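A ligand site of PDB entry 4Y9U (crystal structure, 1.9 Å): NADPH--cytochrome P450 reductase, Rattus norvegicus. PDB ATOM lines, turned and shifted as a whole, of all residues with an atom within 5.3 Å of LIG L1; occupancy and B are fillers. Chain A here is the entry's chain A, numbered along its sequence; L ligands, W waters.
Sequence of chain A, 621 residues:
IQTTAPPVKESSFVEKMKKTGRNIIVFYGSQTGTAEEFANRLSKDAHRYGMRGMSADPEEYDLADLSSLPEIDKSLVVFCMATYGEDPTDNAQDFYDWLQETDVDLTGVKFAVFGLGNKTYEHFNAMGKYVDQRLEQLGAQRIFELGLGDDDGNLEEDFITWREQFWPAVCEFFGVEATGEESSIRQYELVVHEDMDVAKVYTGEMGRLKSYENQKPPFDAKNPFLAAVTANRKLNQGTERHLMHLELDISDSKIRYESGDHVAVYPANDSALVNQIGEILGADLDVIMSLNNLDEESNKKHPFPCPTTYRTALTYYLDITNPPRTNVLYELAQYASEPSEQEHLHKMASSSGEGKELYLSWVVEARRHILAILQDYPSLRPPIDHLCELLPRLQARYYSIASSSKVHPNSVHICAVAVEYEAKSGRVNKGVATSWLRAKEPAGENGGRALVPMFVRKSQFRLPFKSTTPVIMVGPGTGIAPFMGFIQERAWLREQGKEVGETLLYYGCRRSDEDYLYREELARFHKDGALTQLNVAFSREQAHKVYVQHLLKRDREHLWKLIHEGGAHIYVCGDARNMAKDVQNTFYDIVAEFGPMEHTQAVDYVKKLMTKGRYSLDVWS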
ATOM      1  N   GLY A  29      24.901 -16.225 -33.010  1.00  0.00           N
ATOM      2  CA  GLY A  29      24.373 -14.920 -32.686  1.00  0.00           C
ATOM      3  C   GLY A  29      23.862 -15.107 -31.276  1.00  0.00           C
ATOM      4  O   GLY A  29      22.899 -15.843 -31.046  1.00  0.00           O
ATOM      5  N   SER A  30      24.514 -14.445 -30.326  1.00  0.00           N
ATOM      6  CA  SER A  30      24.156 -14.624 -28.931  1.00  0.00           C
ATOM      7  C   SER A  30      24.317 -13.341 -28.115  1.00  0.00           C
ATOM      8  O   SER A  30      25.228 -12.544 -28.360  1.00  0.00           O
ATOM      9  CB  SER A  30      24.983 -15.748 -28.297  1.00  0.00           C
ATOM     10  OG  SER A  30      24.646 -15.970 -26.939  1.00  0.00           O
ATOM     11  N   GLN A  31      23.421 -13.151 -27.151  1.00  0.00           N
ATOM     12  CA  GLN A  31      23.455 -11.983 -26.290  1.00  0.00           C
ATOM     13  C   GLN A  31      23.810 -12.422 -24.861  1.00  0.00           C
ATOM     14  O   GLN A  31      24.667 -11.827 -24.219  1.00  0.00           O
ATOM     15  CB  GLN A  31      22.102 -11.273 -26.299  1.00  0.00           C
ATOM     16  CG  GLN A  31      22.111  -9.909 -25.635  1.00  0.00           C
ATOM     17  CD  GLN A  31      23.036  -8.925 -26.337  1.00  0.00           C
ATOM     18  OE1 GLN A  31      23.190  -8.970 -27.559  1.00  0.00           O
ATOM     19  NE2 GLN A  31      23.656  -8.034 -25.568  1.00  0.00           N
ATOM     20  N   THR A  32      23.151 -13.476 -24.381  1.00  0.00           N
ATOM     21  CA  THR A  32      23.437 -13.977 -23.039  1.00  0.00           C
ATOM     22  C   THR A  32      24.093 -15.354 -23.034  1.00  0.00           C
ATOM     23  O   THR A  32      24.000 -16.111 -22.065  1.00  0.00           O
ATOM     24  CB  THR A  32      22.160 -13.974 -22.167  1.00  0.00           C
ATOM     25  OG1 THR A  32      21.034 -14.402 -22.950  1.00  0.00           O
ATOM     26  CG2 THR A  32      21.894 -12.557 -21.648  1.00  0.00           C
ATOM     27  N   GLY A  33      24.780 -15.674 -24.132  1.00  0.00           N
ATOM     28  CA  GLY A  33      25.512 -16.919 -24.257  1.00  0.00           C
ATOM     29  C   GLY A  33      24.828 -18.246 -24.538  1.00  0.00           C
ATOM     30  O   GLY A  33      25.497 -19.275 -24.471  1.00  0.00           O
ATOM     31  N   THR A  34      23.537 -18.244 -24.843  1.00  0.00           N
ATOM     32  CA  THR A  34      22.853 -19.515 -25.114  1.00  0.00           C
ATOM     33  C   THR A  34      23.202 -20.059 -26.493  1.00  0.00           C
ATOM     34  O   THR A  34      23.606 -21.218 -26.631  1.00  0.00           O
ATOM     35  CB  THR A  34      21.327 -19.387 -25.006  1.00  0.00           C
ATOM     36  OG1 THR A  34      20.991 -18.712 -23.789  1.00  0.00           O
ATOM     37  CG2 THR A  34      20.684 -20.770 -24.992  1.00  0.00           C
ATOM     38  N   ALA A  35      23.051 -19.217 -27.512  1.00  0.00           N
ATOM     39  CA  ALA A  35      23.351 -19.610 -28.884  1.00  0.00           C
ATOM     40  C   ALA A  35      24.840 -19.916 -29.005  1.00  0.00           C
ATOM     41  O   ALA A  35      25.241 -20.781 -29.786  1.00  0.00           O
ATOM     42  CB  ALA A  35      22.959 -18.500 -29.857  1.00  0.00           C
ATOM     43  N   GLU A  36      25.660 -19.214 -28.237  1.00  0.00           N
ATOM     44  CA  GLU A  36      27.097 -19.448 -28.280  1.00  0.00           C
ATOM     45  C   GLU A  36      27.421 -20.853 -27.797  1.00  0.00           C
ATOM     46  O   GLU A  36      28.241 -21.532 -28.409  1.00  0.00           O
ATOM     47  CB  GLU A  36      27.844 -18.409 -27.429  1.00  0.00           C
ATOM     48  CG  GLU A  36      29.302 -18.783 -27.186  1.00  0.00           C
ATOM     49  CD  GLU A  36      30.091 -17.675 -26.512  1.00  0.00           C
ATOM     50  OE1 GLU A  36      29.557 -17.033 -25.566  1.00  0.00           O
ATOM     51  OE2 GLU A  36      31.241 -17.440 -26.919  1.00  0.00           O
ATOM     52  N   ALA A  82      19.946 -16.195 -32.113  1.00  0.00           N
ATOM     53  CA  ALA A  82      18.909 -15.821 -31.162  1.00  0.00           C
ATOM     54  C   ALA A  82      18.393 -14.459 -31.594  1.00  0.00           C
ATOM     55  O   ALA A  82      19.129 -13.693 -32.233  1.00  0.00           O
ATOM     56  CB  ALA A  82      19.485 -15.748 -29.752  1.00  0.00           C
ATOM     57  N   THR A  83      17.163 -14.184 -31.250  1.00  0.00           N
ATOM     58  CA  THR A  83      16.513 -12.929 -31.564  1.00  0.00           C
ATOM     59  C   THR A  83      16.425 -11.909 -30.405  1.00  0.00           C
ATOM     60  O   THR A  83      16.232 -12.316 -29.302  1.00  0.00           O
ATOM     61  CB  THR A  83      15.122 -13.263 -32.028  1.00  0.00           C
ATOM     62  OG1 THR A  83      15.228 -14.066 -33.196  1.00  0.00           O
ATOM     63  CG2 THR A  83      14.304 -12.067 -32.285  1.00  0.00           C
ATOM     64  N   TYR A  84      16.454 -10.622 -30.709  1.00  0.00           N
ATOM     65  CA  TYR A  84      16.168  -9.614 -29.696  1.00  0.00           C
ATOM     66  C   TYR A  84      15.493  -8.391 -30.334  1.00  0.00           C
ATOM     67  O   TYR A  84      15.630  -8.146 -31.532  1.00  0.00           O
ATOM     68  CB  TYR A  84      17.449  -9.175 -28.982  1.00  0.00           C
ATOM     69  CG  TYR A  84      17.970 -10.175 -27.987  1.00  0.00           C
ATOM     70  CD1 TYR A  84      18.488 -11.415 -28.394  1.00  0.00           C
ATOM     71  CD2 TYR A  84      17.939  -9.907 -26.621  1.00  0.00           C
ATOM     72  CE1 TYR A  84      18.937 -12.349 -27.476  1.00  0.00           C
ATOM     73  CE2 TYR A  84      18.393 -10.830 -25.687  1.00  0.00           C
ATOM     74  CZ  TYR A  84      18.902 -12.051 -26.117  1.00  0.00           C
ATOM     75  OH  TYR A  84      19.351 -12.957 -25.193  1.00  0.00           O
ATOM     76  N   THR A  89      20.927  -9.795 -32.726  1.00  0.00           N
ATOM     77  CA  THR A  89      21.860  -9.551 -31.637  1.00  0.00           C
ATOM     78  C   THR A  89      22.949  -8.575 -32.078  1.00  0.00           C
ATOM     79  O   THR A  89      23.256  -8.471 -33.265  1.00  0.00           O
ATOM     80  CB  THR A  89      22.532 -10.855 -31.143  1.00  0.00           C
ATOM     81  OG1 THR A  89      23.203 -11.484 -32.242  1.00  0.00           O
ATOM     82  CG2 THR A  89      21.497 -11.806 -30.572  1.00  0.00           C
ATOM     83  N   LEU A 116      17.024 -19.410 -31.768  1.00  0.00           N
ATOM     84  CA  LEU A 116      16.721 -19.381 -30.336  1.00  0.00           C
ATOM     85  C   LEU A 116      15.757 -18.220 -30.129  1.00  0.00           C
ATOM     86  O   LEU A 116      16.108 -17.069 -30.382  1.00  0.00           O
ATOM     87  CB  LEU A 116      17.969 -19.130 -29.501  1.00  0.00           C
ATOM     88  CG  LEU A 116      19.043 -20.212 -29.404  1.00  0.00           C
ATOM     89  CD1 LEU A 116      19.768 -20.366 -30.735  1.00  0.00           C
ATOM     90  CD2 LEU A 116      20.016 -19.828 -28.302  1.00  0.00           C
ATOM     91  N   GLY A 117      14.538 -18.525 -29.688  1.00  0.00           N
ATOM     92  CA  GLY A 117      13.564 -17.468 -29.467  1.00  0.00           C
ATOM     93  C   GLY A 117      12.737 -17.680 -28.209  1.00  0.00           C
ATOM     94  O   GLY A 117      13.166 -18.357 -27.279  1.00  0.00           O
ATOM     95  N   ASN A 118      11.552 -17.089 -28.209  1.00  0.00           N
ATOM     96  CA  ASN A 118      10.633 -17.190 -27.080  1.00  0.00           C
ATOM     97  C   ASN A 118       9.286 -16.657 -27.560  1.00  0.00           C
ATOM     98  O   ASN A 118       9.156 -15.473 -27.880  1.00  0.00           O
ATOM     99  CB  ASN A 118      11.150 -16.337 -25.909  1.00  0.00           C
ATOM    100  CG  ASN A 118      10.286 -16.471 -24.684  1.00  0.00           C
ATOM    101  OD1 ASN A 118       9.061 -16.426 -24.760  1.00  0.00           O
ATOM    102  ND2 ASN A 118      10.927 -16.626 -23.522  1.00  0.00           N
ATOM    103  N   LYS A 119       8.287 -17.534 -27.612  1.00  0.00           N
ATOM    104  CA  LYS A 119       6.964 -17.151 -28.107  1.00  0.00           C
ATOM    105  C   LYS A 119       6.205 -16.048 -27.374  1.00  0.00           C
ATOM    106  O   LYS A 119       5.327 -15.417 -27.955  1.00  0.00           O
ATOM    107  CB  LYS A 119       6.061 -18.386 -28.209  1.00  0.00           C
ATOM    108  CG  LYS A 119       6.564 -19.427 -29.213  1.00  0.00           C
ATOM    109  CD  LYS A 119       5.497 -20.477 -29.488  1.00  0.00           C
ATOM    110  CE  LYS A 119       6.041 -21.621 -30.328  1.00  0.00           C
ATOM    111  NZ  LYS A 119       7.118 -22.350 -29.584  1.00  0.00           N
ATOM    112  N   TYR A 121       7.137 -13.420 -26.915  1.00  0.00           N
ATOM    113  CA  TYR A 121       7.638 -12.205 -27.551  1.00  0.00           C
ATOM    114  C   TYR A 121       7.091 -12.053 -28.967  1.00  0.00           C
ATOM    115  O   TYR A 121       6.811 -13.043 -29.654  1.00  0.00           O
ATOM    116  CB  TYR A 121       9.178 -12.228 -27.574  1.00  0.00           C
ATOM    117  CG  TYR A 121       9.821 -11.905 -26.238  1.00  0.00           C
ATOM    118  CD1 TYR A 121       9.996 -10.579 -25.838  1.00  0.00           C
ATOM    119  CD2 TYR A 121      10.225 -12.922 -25.372  1.00  0.00           C
ATOM    120  CE1 TYR A 121      10.581 -10.271 -24.613  1.00  0.00           C
ATOM    121  CE2 TYR A 121      10.812 -12.622 -24.142  1.00  0.00           C
ATOM    122  CZ  TYR A 121      10.980 -11.299 -23.763  1.00  0.00           C
ATOM    123  OH  TYR A 121      11.562 -10.996 -22.546  1.00  0.00           O
ATOM    124  N   GLU A 122       6.939 -10.803 -29.404  1.00  0.00           N
ATOM    125  CA  GLU A 122       6.414 -10.490 -30.729  1.00  0.00           C
ATOM    126  C   GLU A 122       6.965 -11.217 -31.948  1.00  0.00           C
ATOM    127  O   GLU A 122       6.265 -12.014 -32.594  1.00  0.00           O
ATOM    128  CB  GLU A 122       6.621  -9.001 -31.041  1.00  0.00           C
ATOM    129  CG  GLU A 122       5.792  -8.061 -30.169  1.00  0.00           C
ATOM    130  CD  GLU A 122       4.307  -8.144 -30.468  1.00  0.00           C
ATOM    131  OE1 GLU A 122       3.513  -7.566 -29.702  1.00  0.00           O
ATOM    132  OE2 GLU A 122       3.929  -8.784 -31.479  1.00  0.00           O
ATOM    133  N   HIS A 123       8.228 -10.929 -32.263  1.00  0.00           N
ATOM    134  CA  HIS A 123       8.914 -11.521 -33.406  1.00  0.00           C
ATOM    135  C   HIS A 123       9.615 -12.795 -32.916  1.00  0.00           C
ATOM    136  O   HIS A 123      10.781 -12.759 -32.537  1.00  0.00           O
ATOM    137  CB  HIS A 123       9.959 -10.556 -33.978  1.00  0.00           C
ATOM    138  CG  HIS A 123       9.398  -9.519 -34.898  1.00  0.00           C
ATOM    139  ND1 HIS A 123       9.186  -8.213 -34.518  1.00  0.00           N
ATOM    140  CD2 HIS A 123       8.981  -9.602 -36.185  1.00  0.00           C
ATOM    141  CE1 HIS A 123       8.677  -7.535 -35.526  1.00  0.00           C
ATOM    142  NE2 HIS A 123       8.535  -8.353 -36.556  1.00  0.00           N
ATOM    143  N   PHE A 124       8.902 -13.904 -32.939  1.00  0.00           N
ATOM    144  CA  PHE A 124       9.462 -15.183 -32.492  1.00  0.00           C
ATOM    145  C   PHE A 124      10.466 -15.773 -33.479  1.00  0.00           C
ATOM    146  O   PHE A 124      10.112 -16.155 -34.595  1.00  0.00           O
ATOM    147  CB  PHE A 124       8.330 -16.203 -32.273  1.00  0.00           C
ATOM    148  CG  PHE A 124       8.817 -17.569 -31.893  1.00  0.00           C
ATOM    149  CD1 PHE A 124       9.556 -17.769 -30.729  1.00  0.00           C
ATOM    150  CD2 PHE A 124       8.560 -18.663 -32.715  1.00  0.00           C
ATOM    151  CE1 PHE A 124      10.024 -19.033 -30.392  1.00  0.00           C
ATOM    152  CE2 PHE A 124       9.016 -19.933 -32.382  1.00  0.00           C
ATOM    153  CZ  PHE A 124       9.755 -20.119 -31.215  1.00  0.00           C
ATOM    154  N   ASN A 125      11.731 -15.856 -33.044  1.00  0.00           N
ATOM    155  CA  ASN A 125      12.804 -16.395 -33.886  1.00  0.00           C
ATOM    156  C   ASN A 125      12.924 -15.664 -35.213  1.00  0.00           C
ATOM    157  O   ASN A 125      13.216 -16.280 -36.243  1.00  0.00           O
ATOM    158  CB  ASN A 125      12.582 -17.884 -34.140  1.00  0.00           C
ATOM    159  CG  ASN A 125      13.199 -18.757 -33.063  1.00  0.00           C
ATOM    160  OD1 ASN A 125      14.339 -18.542 -32.640  1.00  0.00           O
ATOM    161  ND2 ASN A 125      12.453 -19.768 -32.613  1.00  0.00           N
ATOM    162  N   ALA A 126      12.719 -14.359 -35.178  1.00  0.00           N
ATOM    163  CA  ALA A 126      12.793 -13.536 -36.379  1.00  0.00           C
ATOM    164  C   ALA A 126      14.160 -13.659 -37.040  1.00  0.00           C
ATOM    165  O   ALA A 126      14.246 -13.908 -38.246  1.00  0.00           O
ATOM    166  CB  ALA A 126      12.505 -12.070 -36.040  1.00  0.00           C
ATOM    167  N   ASP A 151      12.219 -20.817 -25.848  1.00  0.00           N
ATOM    168  CA  ASP A 151      12.647 -20.716 -24.463  1.00  0.00           C
ATOM    169  C   ASP A 151      11.465 -20.619 -23.485  1.00  0.00           C
ATOM    170  O   ASP A 151      11.654 -20.651 -22.262  1.00  0.00           O
ATOM    171  CB  ASP A 151      13.564 -19.488 -24.322  1.00  0.00           C
ATOM    172  CG  ASP A 151      14.401 -19.514 -23.060  1.00  0.00           C
ATOM    173  OD1 ASP A 151      14.973 -20.584 -22.730  1.00  0.00           O
ATOM    174  OD2 ASP A 151      14.512 -18.461 -22.393  1.00  0.00           O
ATOM    175  N   LEU A 155      13.959 -24.733 -24.430  1.00  0.00           N
ATOM    176  CA  LEU A 155      14.912 -24.542 -25.508  1.00  0.00           C
ATOM    177  C   LEU A 155      15.932 -25.667 -25.605  1.00  0.00           C
ATOM    178  O   LEU A 155      16.209 -26.164 -26.691  1.00  0.00           O
ATOM    179  CB  LEU A 155      15.627 -23.205 -25.320  1.00  0.00           C
ATOM    180  CG  LEU A 155      16.670 -22.829 -26.356  1.00  0.00           C
ATOM    181  CD1 LEU A 155      16.033 -22.832 -27.747  1.00  0.00           C
ATOM    182  CD2 LEU A 155      17.232 -21.453 -26.022  1.00  0.00           C
ATOM    183  N   VAL A 619      10.292  -5.241 -21.459  1.00  0.00           N
ATOM    184  CA  VAL A 619       9.797  -6.319 -20.630  1.00  0.00           C
ATOM    185  C   VAL A 619      10.804  -7.455 -20.550  1.00  0.00           C
ATOM    186  O   VAL A 619      11.639  -7.629 -21.443  1.00  0.00           O
ATOM    187  CB  VAL A 619       8.457  -6.864 -21.161  1.00  0.00           C
ATOM    188  CG1 VAL A 619       7.379  -5.809 -20.995  1.00  0.00           C
ATOM    189  CG2 VAL A 619       8.581  -7.255 -22.645  1.00  0.00           C
HETATM  190  N1  LIG L   1      12.802 -14.080 -28.490  1.00  0.00           N
HETATM  191  C1  LIG L   1      12.131 -13.960 -29.655  1.00  0.00           C
HETATM  192  O1  LIG L   1      11.825 -14.945 -30.324  1.00  0.00           O
HETATM  193  N2  LIG L   1      11.819 -12.671 -30.058  1.00  0.00           N
HETATM  194  C2  LIG L   1      12.114 -11.470 -29.390  1.00  0.00           C
HETATM  195  O2  LIG L   1      11.723 -10.454 -29.940  1.00  0.00           O
HETATM  196  C3  LIG L   1      12.799 -11.589 -28.153  1.00  0.00           C
HETATM  197  N3  LIG L   1      13.098 -10.410 -27.444  1.00  0.00           N
HETATM  198  C4  LIG L   1      13.775 -10.616 -26.245  1.00  0.00           C
HETATM  199  C5  LIG L   1      14.079  -9.430 -25.491  1.00  0.00           C
HETATM  200  C6  LIG L   1      14.755  -9.495 -24.241  1.00  0.00           C
HETATM  201  C7  LIG L   1      15.005  -8.137 -23.556  1.00  0.00           C
HETATM  202  C8  LIG L   1      15.170 -10.817 -23.667  1.00  0.00           C
HETATM  203  C9  LIG L   1      15.835 -11.015 -22.469  1.00  0.00           C
HETATM  204  C10 LIG L   1      14.888 -11.973 -24.385  1.00  0.00           C
HETATM  205  C11 LIG L   1      14.185 -11.922 -25.681  1.00  0.00           C
HETATM  206  N4  LIG L   1      13.842 -13.103 -26.489  1.00  0.00           N
HETATM  207  C12 LIG L   1      13.117 -12.939 -27.771  1.00  0.00           C
HETATM  208  C13 LIG L   1      14.200 -14.457 -26.054  1.00  0.00           C
HETATM  209  C14 LIG L   1      15.616 -14.911 -26.528  1.00  0.00           C
HETATM  210  O3  LIG L   1      15.657 -14.870 -28.006  1.00  0.00           O
HETATM  211  C15 LIG L   1      15.912 -16.317 -26.035  1.00  0.00           C
HETATM  212  O4  LIG L   1      15.868 -16.280 -24.587  1.00  0.00           O
HETATM  213  C16 LIG L   1      17.346 -16.756 -26.551  1.00  0.00           C
HETATM  214  O5  LIG L   1      17.430 -18.110 -26.019  1.00  0.00           O
HETATM  215  C17 LIG L   1      18.497 -15.977 -25.916  1.00  0.00           C
HETATM  216  O6  LIG L   1      19.837 -16.401 -26.426  1.00  0.00           O
HETATM  217  P1  LIG L   1      21.253 -15.841 -25.981  1.00  0.00           P
HETATM  218  O7  LIG L   1      21.555 -16.211 -24.573  1.00  0.00           O
HETATM  219  O8  LIG L   1      21.215 -14.333 -26.385  1.00  0.00           O
HETATM  220  O9  LIG L   1      22.220 -16.697 -26.930  1.00  0.00           O
HETATM  221  P1  LG2 L   2      19.471 -15.186 -11.203  1.00  0.00           P
HETATM  222  O1  LG2 L   2      20.478 -15.849 -10.346  1.00  0.00           O
HETATM  223  O2  LG2 L   2      19.860 -14.741 -12.559  1.00  0.00           O
HETATM  224  O3  LG2 L   2      18.190 -16.155 -11.318  1.00  0.00           O
HETATM  225  C1  LG2 L   2      17.094 -15.807 -12.174  1.00  0.00           C
HETATM  226  C2  LG2 L   2      16.274 -17.063 -12.439  1.00  0.00           C
HETATM  227  O4  LG2 L   2      15.735 -17.588 -11.222  1.00  0.00           O
HETATM  228  C3  LG2 L   2      15.012 -16.768 -13.232  1.00  0.00           C
HETATM  229  O5  LG2 L   2      15.365 -16.606 -14.614  1.00  0.00           O
HETATM  230  C4  LG2 L   2      14.329 -18.104 -13.050  1.00  0.00           C
HETATM  231  O6  LG2 L   2      14.927 -19.070 -13.920  1.00  0.00           O
HETATM  232  C5  LG2 L   2      14.645 -18.453 -11.598  1.00  0.00           C
HETATM  233  N1  LG2 L   2      13.530 -18.134 -10.699  1.00  0.00           N
HETATM  234  C6  LG2 L   2      13.180 -16.799 -10.158  1.00  0.00           C
HETATM  235  N2  LG2 L   2      12.021 -17.154  -9.305  1.00  0.00           N
HETATM  236  C7  LG2 L   2      11.805 -18.459  -9.389  1.00  0.00           C
HETATM  237  C8  LG2 L   2      10.877 -19.202  -8.785  1.00  0.00           C
HETATM  238  N3  LG2 L   2      10.091 -18.562  -7.925  1.00  0.00           N
HETATM  239  N4  LG2 L   2      10.705 -20.502  -9.051  1.00  0.00           N
HETATM  240  C9  LG2 L   2      11.529 -21.109 -10.009  1.00  0.00           C
HETATM  241  N5  LG2 L   2      12.475 -20.296 -10.644  1.00  0.00           N
HETATM  242  C10 LG2 L   2      12.595 -19.007 -10.316  1.00  0.00           C
HETATM  243  N6  LG2 L   2      15.027  -6.792 -12.943  1.00  0.00           N
HETATM  244  C11 LG2 L   2      14.692  -5.831 -11.984  1.00  0.00           C
HETATM  245  O7  LG2 L   2      14.430  -6.189 -10.832  1.00  0.00           O
HETATM  246  N7  LG2 L   2      14.591  -4.487 -12.352  1.00  0.00           N
HETATM  247  C12 LG2 L   2      14.827  -4.097 -13.671  1.00  0.00           C
HETATM  248  O8  LG2 L   2      14.836  -2.900 -13.954  1.00  0.00           O
HETATM  249  C13 LG2 L   2      15.142  -5.059 -14.624  1.00  0.00           C
HETATM  250  N8  LG2 L   2      15.238  -4.707 -15.924  1.00  0.00           N
HETATM  251  C14 LG2 L   2      15.553  -5.632 -16.840  1.00  0.00           C
HETATM  252  C15 LG2 L   2      15.735  -5.248 -18.164  1.00  0.00           C
HETATM  253  C16 LG2 L   2      16.135  -6.183 -19.111  1.00  0.00           C
HETATM  254  C17 LG2 L   2      16.430  -5.762 -20.407  1.00  0.00           C
HETATM  255  C18 LG2 L   2      16.333  -7.508 -18.736  1.00  0.00           C
HETATM  256  C19 LG2 L   2      16.748  -8.445 -19.673  1.00  0.00           C
HETATM  257  C20 LG2 L   2      16.150  -7.884 -17.417  1.00  0.00           C
HETATM  258  C21 LG2 L   2      15.785  -6.945 -16.458  1.00  0.00           C
HETATM  259  N9  LG2 L   2      15.675  -7.294 -15.168  1.00  0.00           N
HETATM  260  C22 LG2 L   2      15.236  -6.392 -14.274  1.00  0.00           C
HETATM  261  C23 LG2 L   2      15.935  -8.686 -14.713  1.00  0.00           C
HETATM  262  C24 LG2 L   2      17.391  -8.813 -14.254  1.00  0.00           C
HETATM  263  O9  LG2 L   2      18.257  -8.662 -15.378  1.00  0.00           O
HETATM  264  C25 LG2 L   2      17.666 -10.170 -13.599  1.00  0.00           C
HETATM  265  O10 LG2 L   2      17.228 -11.235 -14.450  1.00  0.00           O
HETATM  266  C26 LG2 L   2      16.975 -10.281 -12.240  1.00  0.00           C
HETATM  267  O11 LG2 L   2      17.352  -9.183 -11.407  1.00  0.00           O
HETATM  268  C27 LG2 L   2      17.393 -11.595 -11.559  1.00  0.00           C
HETATM  269  O12 LG2 L   2      18.818 -11.693 -11.556  1.00  0.00           O
HETATM  270  P2  LG2 L   2      19.605 -12.509 -10.406  1.00  0.00           P
HETATM  271  O13 LG2 L   2      19.353 -11.853  -9.100  1.00  0.00           O
HETATM  272  O14 LG2 L   2      21.005 -12.673 -10.857  1.00  0.00           O
HETATM  273  O15 LG2 L   2      18.853 -13.932 -10.407  1.00  0.00           O
HETATM  274  O   HOH W   1      18.526 -18.646 -22.942  1.00  0.00           O
HETATM  275  O   HOH W   2      18.128  -7.772 -23.531  1.00  0.00           O
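O8 of LIG L1 is in hydrogen-bond range of N of Thr 32 (2.9 Å). OG1 of Thr 32 is in hydrogen-bond range of O7 of LIG L1. The side-chain hydroxyl of Ser 30 is in hydrogen-bond range of an oxygen (O9) of LIG L1, at 2.5 Å. An oxygen (O8) of LIG L1 lies within hydrogen-bond range of the side-chain hydroxyl (OH) of Tyr 84 (2.6 Å). The backbone NH of Gln 31 sits at hydrogen-bond distance from an oxygen (O8) of LIG L1 (2.6 Å). O7 of LIG L1 sits at hydrogen-bond distance from N of Thr 34, at 2.9 Å. The side-chain hydroxyl (OG1) of Thr 34 lies within hydrogen-bond range of an oxygen (O7) of LIG L1 (2.7 Å). O of His 123 lies within hydrogen-bond range of N2 of LIG L1 (2.7 Å). N of Ala 35 lies within hydrogen-bond range of O9 of LIG L1, 2.7 Å away. An oxygen (O1) of LIG L1 is in hydrogen-bond range of the backbone NH (N) of Asn 125 (2.9 Å). O of Thr 83 is in hydrogen-bond range of O3 of LIG L1, 2.9 Å away. An oxygen (O1) of LIG L1 sits at hydrogen-bond distance from the backbone NH (N) of Asn 118. O3 of LIG L1 is in hydrogen-bond range of O of Leu 116 (3.3 Å). An oxygen (O7) of LIG L1 sits at hydrogen-bond distance from the backbone NH (N) of Gly 33, at 3.3 Å. OD2 of Asp 151 sits at hydrogen-bond distance from O4 of LIG L1.
The side-chain hydroxyl of Tyr 84 lies within hydrogen-bond range of the side-chain hydroxyl of Thr 32. OG of Ser 30 is in hydrogen-bond range of N of Thr 34. The side-chain amide oxygen of Asn 125 is in hydrogen-bond range of the backbone NH of Gly 117 (3.0 Å). OD1 of Asn 125 sits close to N of Leu 116 (3.0 Å). O of Leu 116 sits at hydrogen-bond distance from N of Thr 83 (3.2 Å). N of Ala 126 is in hydrogen-bond range of OG1 of Thr 83 (3.2 Å). The backbone carbonyl oxygen (O) of Gly 117 lies within hydrogen-bond range of the backbone NH (N) of Asp 151 (3.0 Å). The backbone NH (N) of Ala 82 is in hydrogen-bond range of the backbone carbonyl oxygen (O) of Gly 29, 3.2 Å away.
Ala 82 touches LIG L1. Gly 117 touches LIG L1. Tyr 121 touches LIG L1 (CD1 to N3, 3.5 Å). Phe 124 touches LIG L1. Leu 155 touches LIG L1 (CD2 to O5, 3.3 Å). Hydrophobic or aromatic side chains within 4 Å of LIG L1: Ala 35, Ala 82, Tyr 84, Leu 116, Tyr 121, Phe 124 and Leu 155.
Water W1 lies within hydrogen-bond range of OG1 of Thr 34 (2.6 Å) and O5 of LIG L1 (3.3 Å).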
